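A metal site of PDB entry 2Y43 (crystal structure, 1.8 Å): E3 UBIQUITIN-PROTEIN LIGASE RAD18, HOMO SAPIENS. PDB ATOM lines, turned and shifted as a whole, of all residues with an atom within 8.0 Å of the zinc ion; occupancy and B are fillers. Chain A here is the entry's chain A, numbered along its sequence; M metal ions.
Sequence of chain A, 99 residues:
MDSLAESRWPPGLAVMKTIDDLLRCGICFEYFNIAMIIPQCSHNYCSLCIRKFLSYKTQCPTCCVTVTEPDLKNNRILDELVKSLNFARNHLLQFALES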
ATOM      1  N   ARG A  24     -12.425 -33.417 -22.788  1.00  0.00           N
ATOM      2  CA  ARG A  24     -13.048 -32.638 -21.722  1.00  0.00           C
ATOM      3  C   ARG A  24     -12.001 -32.057 -20.782  1.00  0.00           C
ATOM      4  O   ARG A  24     -11.143 -32.781 -20.293  1.00  0.00           O
ATOM      5  CB  ARG A  24     -14.010 -33.507 -20.906  1.00  0.00           C
ATOM      6  CG  ARG A  24     -15.372 -33.672 -21.527  1.00  0.00           C
ATOM      7  CD  ARG A  24     -16.402 -34.187 -20.519  1.00  0.00           C
ATOM      8  NE  ARG A  24     -17.628 -34.537 -21.220  1.00  0.00           N
ATOM      9  CZ  ARG A  24     -18.578 -33.673 -21.560  1.00  0.00           C
ATOM     10  NH1 ARG A  24     -18.453 -32.377 -21.253  1.00  0.00           N
ATOM     11  NH2 ARG A  24     -19.657 -34.095 -22.204  1.00  0.00           N
ATOM     12  N   CYS A  25     -12.094 -30.758 -20.518  1.00  0.00           N
ATOM     13  CA  CYS A  25     -11.190 -30.071 -19.587  1.00  0.00           C
ATOM     14  C   CYS A  25     -11.457 -30.538 -18.167  1.00  0.00           C
ATOM     15  O   CYS A  25     -12.600 -30.592 -17.734  1.00  0.00           O
ATOM     16  CB  CYS A  25     -11.423 -28.564 -19.683  1.00  0.00           C
ATOM     17  SG  CYS A  25     -10.556 -27.578 -18.463  1.00  0.00           S
ATOM     18  N   GLY A  26     -10.391 -30.889 -17.456  1.00  0.00           N
ATOM     19  CA  GLY A  26     -10.516 -31.432 -16.108  1.00  0.00           C
ATOM     20  C   GLY A  26     -10.821 -30.362 -15.056  1.00  0.00           C
ATOM     21  O   GLY A  26     -11.091 -30.682 -13.903  1.00  0.00           O
ATOM     22  N   ILE A  27     -10.777 -29.101 -15.469  1.00  0.00           N
ATOM     23  CA  ILE A  27     -11.110 -28.008 -14.557  1.00  0.00           C
ATOM     24  C   ILE A  27     -12.564 -27.569 -14.654  1.00  0.00           C
ATOM     25  O   ILE A  27     -13.259 -27.460 -13.634  1.00  0.00           O
ATOM     26  CB  ILE A  27     -10.162 -26.800 -14.754  1.00  0.00           C
ATOM     27  CG1 ILE A  27      -8.784 -27.143 -14.196  1.00  0.00           C
ATOM     28  CG2 ILE A  27     -10.697 -25.565 -13.999  1.00  0.00           C
ATOM     29  CD1 ILE A  27      -7.715 -26.164 -14.632  1.00  0.00           C
ATOM     30  N   CYS A  28     -13.042 -27.337 -15.885  1.00  0.00           N
ATOM     31  CA  CYS A  28     -14.427 -26.854 -16.075  1.00  0.00           C
ATOM     32  C   CYS A  28     -15.397 -27.946 -16.507  1.00  0.00           C
ATOM     33  O   CYS A  28     -16.610 -27.735 -16.486  1.00  0.00           O
ATOM     34  CB  CYS A  28     -14.467 -25.706 -17.100  1.00  0.00           C
ATOM     35  SG  CYS A  28     -14.034 -26.245 -18.784  1.00  0.00           S
ATOM     36  N   PHE A  29     -14.868 -29.101 -16.915  1.00  0.00           N
ATOM     37  CA  PHE A  29     -15.683 -30.234 -17.367  1.00  0.00           C
ATOM     38  C   PHE A  29     -16.442 -29.995 -18.700  1.00  0.00           C
ATOM     39  O   PHE A  29     -17.436 -30.683 -19.007  1.00  0.00           O
ATOM     40  CB  PHE A  29     -16.644 -30.687 -16.251  1.00  0.00           C
ATOM     41  CG  PHE A  29     -16.760 -32.176 -16.122  1.00  0.00           C
ATOM     42  CD1 PHE A  29     -15.665 -32.935 -15.707  1.00  0.00           C
ATOM     43  CD2 PHE A  29     -17.956 -32.822 -16.428  1.00  0.00           C
ATOM     44  CE1 PHE A  29     -15.767 -34.322 -15.582  1.00  0.00           C
ATOM     45  CE2 PHE A  29     -18.064 -34.209 -16.316  1.00  0.00           C
ATOM     46  CZ  PHE A  29     -16.963 -34.956 -15.894  1.00  0.00           C
ATOM     47  N   GLU A  30     -15.968 -29.017 -19.472  1.00  0.00           N
ATOM     48  CA  GLU A  30     -16.518 -28.753 -20.802  1.00  0.00           C
ATOM     49  C   GLU A  30     -15.470 -29.134 -21.821  1.00  0.00           C
ATOM     50  O   GLU A  30     -14.304 -29.283 -21.474  1.00  0.00           O
ATOM     51  CB  GLU A  30     -16.862 -27.255 -20.969  1.00  0.00           C
ATOM     52  CG  GLU A  30     -17.803 -26.670 -19.933  1.00  0.00           C
ATOM     53  CD  GLU A  30     -19.252 -27.163 -20.048  1.00  0.00           C
ATOM     54  OE1 GLU A  30     -19.590 -27.896 -21.002  1.00  0.00           O
ATOM     55  OE2 GLU A  30     -20.064 -26.800 -19.178  1.00  0.00           O
ATOM     56  N   TYR A  31     -15.863 -29.276 -23.085  1.00  0.00           N
ATOM     57  CA  TYR A  31     -14.879 -29.564 -24.131  1.00  0.00           C
ATOM     58  C   TYR A  31     -13.886 -28.406 -24.190  1.00  0.00           C
ATOM     59  O   TYR A  31     -14.280 -27.251 -23.965  1.00  0.00           O
ATOM     60  CB  TYR A  31     -15.566 -29.771 -25.482  1.00  0.00           C
ATOM     61  CG  TYR A  31     -16.512 -30.959 -25.460  1.00  0.00           C
ATOM     62  CD1 TYR A  31     -16.044 -32.231 -25.115  1.00  0.00           C
ATOM     63  CD2 TYR A  31     -17.848 -30.812 -25.809  1.00  0.00           C
ATOM     64  CE1 TYR A  31     -16.923 -33.336 -25.080  1.00  0.00           C
ATOM     65  CE2 TYR A  31     -18.709 -31.900 -25.773  1.00  0.00           C
ATOM     66  CZ  TYR A  31     -18.247 -33.154 -25.423  1.00  0.00           C
ATOM     67  OH  TYR A  31     -19.124 -34.233 -25.402  1.00  0.00           O
ATOM     68  N   PHE A  32     -12.626 -28.719 -24.446  1.00  0.00           N
ATOM     69  CA  PHE A  32     -11.556 -27.708 -24.459  1.00  0.00           C
ATOM     70  C   PHE A  32     -11.924 -26.505 -25.302  1.00  0.00           C
ATOM     71  O   PHE A  32     -12.410 -26.675 -26.432  1.00  0.00           O
ATOM     72  CB  PHE A  32     -10.254 -28.280 -25.032  1.00  0.00           C
ATOM     73  CG  PHE A  32      -9.656 -29.398 -24.234  1.00  0.00           C
ATOM     74  CD1 PHE A  32      -9.214 -29.176 -22.921  1.00  0.00           C
ATOM     75  CD2 PHE A  32      -9.502 -30.673 -24.795  1.00  0.00           C
ATOM     76  CE1 PHE A  32      -8.653 -30.207 -22.175  1.00  0.00           C
ATOM     77  CE2 PHE A  32      -8.947 -31.715 -24.056  1.00  0.00           C
ATOM     78  CZ  PHE A  32      -8.521 -31.490 -22.736  1.00  0.00           C
ATOM     79  N   ASN A  33     -11.691 -25.316 -24.750  1.00  0.00           N
ATOM     80  CA  ASN A  33     -11.763 -24.039 -25.490  1.00  0.00           C
ATOM     81  C   ASN A  33     -10.386 -23.401 -25.363  1.00  0.00           C
ATOM     82  O   ASN A  33      -9.977 -23.024 -24.258  1.00  0.00           O
ATOM     83  CB  ASN A  33     -12.840 -23.134 -24.874  1.00  0.00           C
ATOM     84  CG  ASN A  33     -12.827 -21.709 -25.434  1.00  0.00           C
ATOM     85  OD1 ASN A  33     -12.952 -21.508 -26.633  1.00  0.00           O
ATOM     86  ND2 ASN A  33     -12.684 -20.701 -24.551  1.00  0.00           N
ATOM     87  N   ILE A  34      -9.688 -23.279 -26.492  1.00  0.00           N
ATOM     88  CA  ILE A  34      -8.297 -22.827 -26.519  1.00  0.00           C
ATOM     89  C   ILE A  34      -7.427 -23.737 -25.624  1.00  0.00           C
ATOM     90  O   ILE A  34      -6.912 -23.326 -24.566  1.00  0.00           O
ATOM     91  CB  ILE A  34      -8.105 -21.333 -26.135  1.00  0.00           C
ATOM     92  CG1 ILE A  34      -9.201 -20.445 -26.743  1.00  0.00           C
ATOM     93  CG2 ILE A  34      -6.694 -20.865 -26.627  1.00  0.00           C
ATOM     94  CD1 ILE A  34      -9.103 -18.992 -26.310  1.00  0.00           C
ATOM     95  N   ASN A  44      -3.655 -31.284 -20.324  1.00  0.00           N
ATOM     96  CA  ASN A  44      -4.250 -30.205 -21.090  1.00  0.00           C
ATOM     97  C   ASN A  44      -5.482 -29.630 -20.383  1.00  0.00           C
ATOM     98  O   ASN A  44      -6.255 -30.373 -19.752  1.00  0.00           O
ATOM     99  CB  ASN A  44      -4.720 -30.716 -22.451  1.00  0.00           C
ATOM    100  CG  ASN A  44      -3.590 -31.299 -23.271  1.00  0.00           C
ATOM    101  OD1 ASN A  44      -2.819 -30.563 -23.871  1.00  0.00           O
ATOM    102  ND2 ASN A  44      -3.498 -32.608 -23.299  1.00  0.00           N
ATOM    103  N   TYR A  45      -5.660 -28.319 -20.528  1.00  0.00           N
ATOM    104  CA  TYR A  45      -6.791 -27.565 -19.943  1.00  0.00           C
ATOM    105  C   TYR A  45      -7.137 -26.402 -20.860  1.00  0.00           C
ATOM    106  O   TYR A  45      -6.285 -25.968 -21.629  1.00  0.00           O
ATOM    107  CB  TYR A  45      -6.430 -26.953 -18.567  1.00  0.00           C
ATOM    108  CG  TYR A  45      -5.982 -28.025 -17.620  1.00  0.00           C
ATOM    109  CD1 TYR A  45      -6.929 -28.784 -16.929  1.00  0.00           C
ATOM    110  CD2 TYR A  45      -4.644 -28.326 -17.486  1.00  0.00           C
ATOM    111  CE1 TYR A  45      -6.526 -29.824 -16.091  1.00  0.00           C
ATOM    112  CE2 TYR A  45      -4.228 -29.373 -16.646  1.00  0.00           C
ATOM    113  CZ  TYR A  45      -5.165 -30.106 -15.964  1.00  0.00           C
ATOM    114  OH  TYR A  45      -4.741 -31.109 -15.162  1.00  0.00           O
ATOM    115  N   CYS A  46      -8.366 -25.899 -20.773  1.00  0.00           N
ATOM    116  CA  CYS A  46      -8.708 -24.630 -21.444  1.00  0.00           C
ATOM    117  C   CYS A  46      -7.745 -23.586 -20.907  1.00  0.00           C
ATOM    118  O   CYS A  46      -7.401 -23.626 -19.718  1.00  0.00           O
ATOM    119  CB  CYS A  46     -10.107 -24.152 -21.116  1.00  0.00           C
ATOM    120  SG  CYS A  46     -11.368 -25.359 -21.323  1.00  0.00           S
ATOM    121  N   SER A  47      -7.317 -22.684 -21.783  1.00  0.00           N
ATOM    122  CA  SER A  47      -6.373 -21.640 -21.413  1.00  0.00           C
ATOM    123  C   SER A  47      -6.796 -20.854 -20.182  1.00  0.00           C
ATOM    124  O   SER A  47      -6.017 -20.717 -19.241  1.00  0.00           O
ATOM    125  CB  SER A  47      -6.165 -20.661 -22.568  1.00  0.00           C
ATOM    126  OG  SER A  47      -5.253 -19.639 -22.196  1.00  0.00           O
ATOM    127  N   LEU A  48      -8.029 -20.356 -20.178  1.00  0.00           N
ATOM    128  CA  LEU A  48      -8.507 -19.560 -19.069  1.00  0.00           C
ATOM    129  C   LEU A  48      -8.572 -20.386 -17.765  1.00  0.00           C
ATOM    130  O   LEU A  48      -8.210 -19.895 -16.707  1.00  0.00           O
ATOM    131  CB  LEU A  48      -9.854 -18.906 -19.387  1.00  0.00           C
ATOM    132  CG  LEU A  48     -10.502 -18.023 -18.293  1.00  0.00           C
ATOM    133  CD1 LEU A  48      -9.577 -16.893 -17.855  1.00  0.00           C
ATOM    134  CD2 LEU A  48     -11.807 -17.488 -18.830  1.00  0.00           C
ATOM    135  N   CYS A  49      -9.041 -21.622 -17.884  1.00  0.00           N
ATOM    136  CA  CYS A  49      -9.223 -22.507 -16.729  1.00  0.00           C
ATOM    137  C   CYS A  49      -7.907 -22.688 -15.978  1.00  0.00           C
ATOM    138  O   CYS A  49      -7.836 -22.457 -14.769  1.00  0.00           O
ATOM    139  CB  CYS A  49      -9.768 -23.861 -17.196  1.00  0.00           C
ATOM    140  SG  CYS A  49     -11.458 -23.743 -17.781  1.00  0.00           S
ATOM    141  N   ILE A  50      -6.862 -23.070 -16.714  1.00  0.00           N
ATOM    142  CA  ILE A  50      -5.572 -23.347 -16.100  1.00  0.00           C
ATOM    143  C   ILE A  50      -4.872 -22.077 -15.612  1.00  0.00           C
ATOM    144  O   ILE A  50      -4.282 -22.078 -14.524  1.00  0.00           O
ATOM    145  CB  ILE A  50      -4.657 -24.291 -16.969  1.00  0.00           C
ATOM    146  CG1 ILE A  50      -3.368 -24.664 -16.219  1.00  0.00           C
ATOM    147  CG2 ILE A  50      -4.345 -23.676 -18.362  1.00  0.00           C
ATOM    148  CD1 ILE A  50      -3.598 -25.429 -14.904  1.00  0.00           C
HETATM  149 ZN    ZN M   1     -11.848 -25.724 -19.005  1.00  0.00          ZN
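Within 4 Å of the zinc ion: Cys 25, Cys 28, Cys 46 and Cys 49.
The nearest printed residue that does not touch the zinc ion is Ile 27 (4.7 Å).
N of Glu 30 lies close to SG of Cys 28 (3.4 Å).
N of Cys 25 lies within hydrogen-bond range of O of Glu 30 (2.8 Å).
SG of Cys 25 lies close to N of Ile 27, 3.4 Å away.
SG of Cys 46 sits close to N of Asn 33 (3.4 Å).
The zinc ion is bound by the side-chain sulfur of Cys 28 (2.3 Å), the side-chain sulfur of Cys 25 (2.3 Å), the side-chain sulfur of Cys 49 (2.4 Å) and the side-chain sulfur of Cys 46 (2.4 Å).
The zinc ion has four donor atoms within binding distance.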
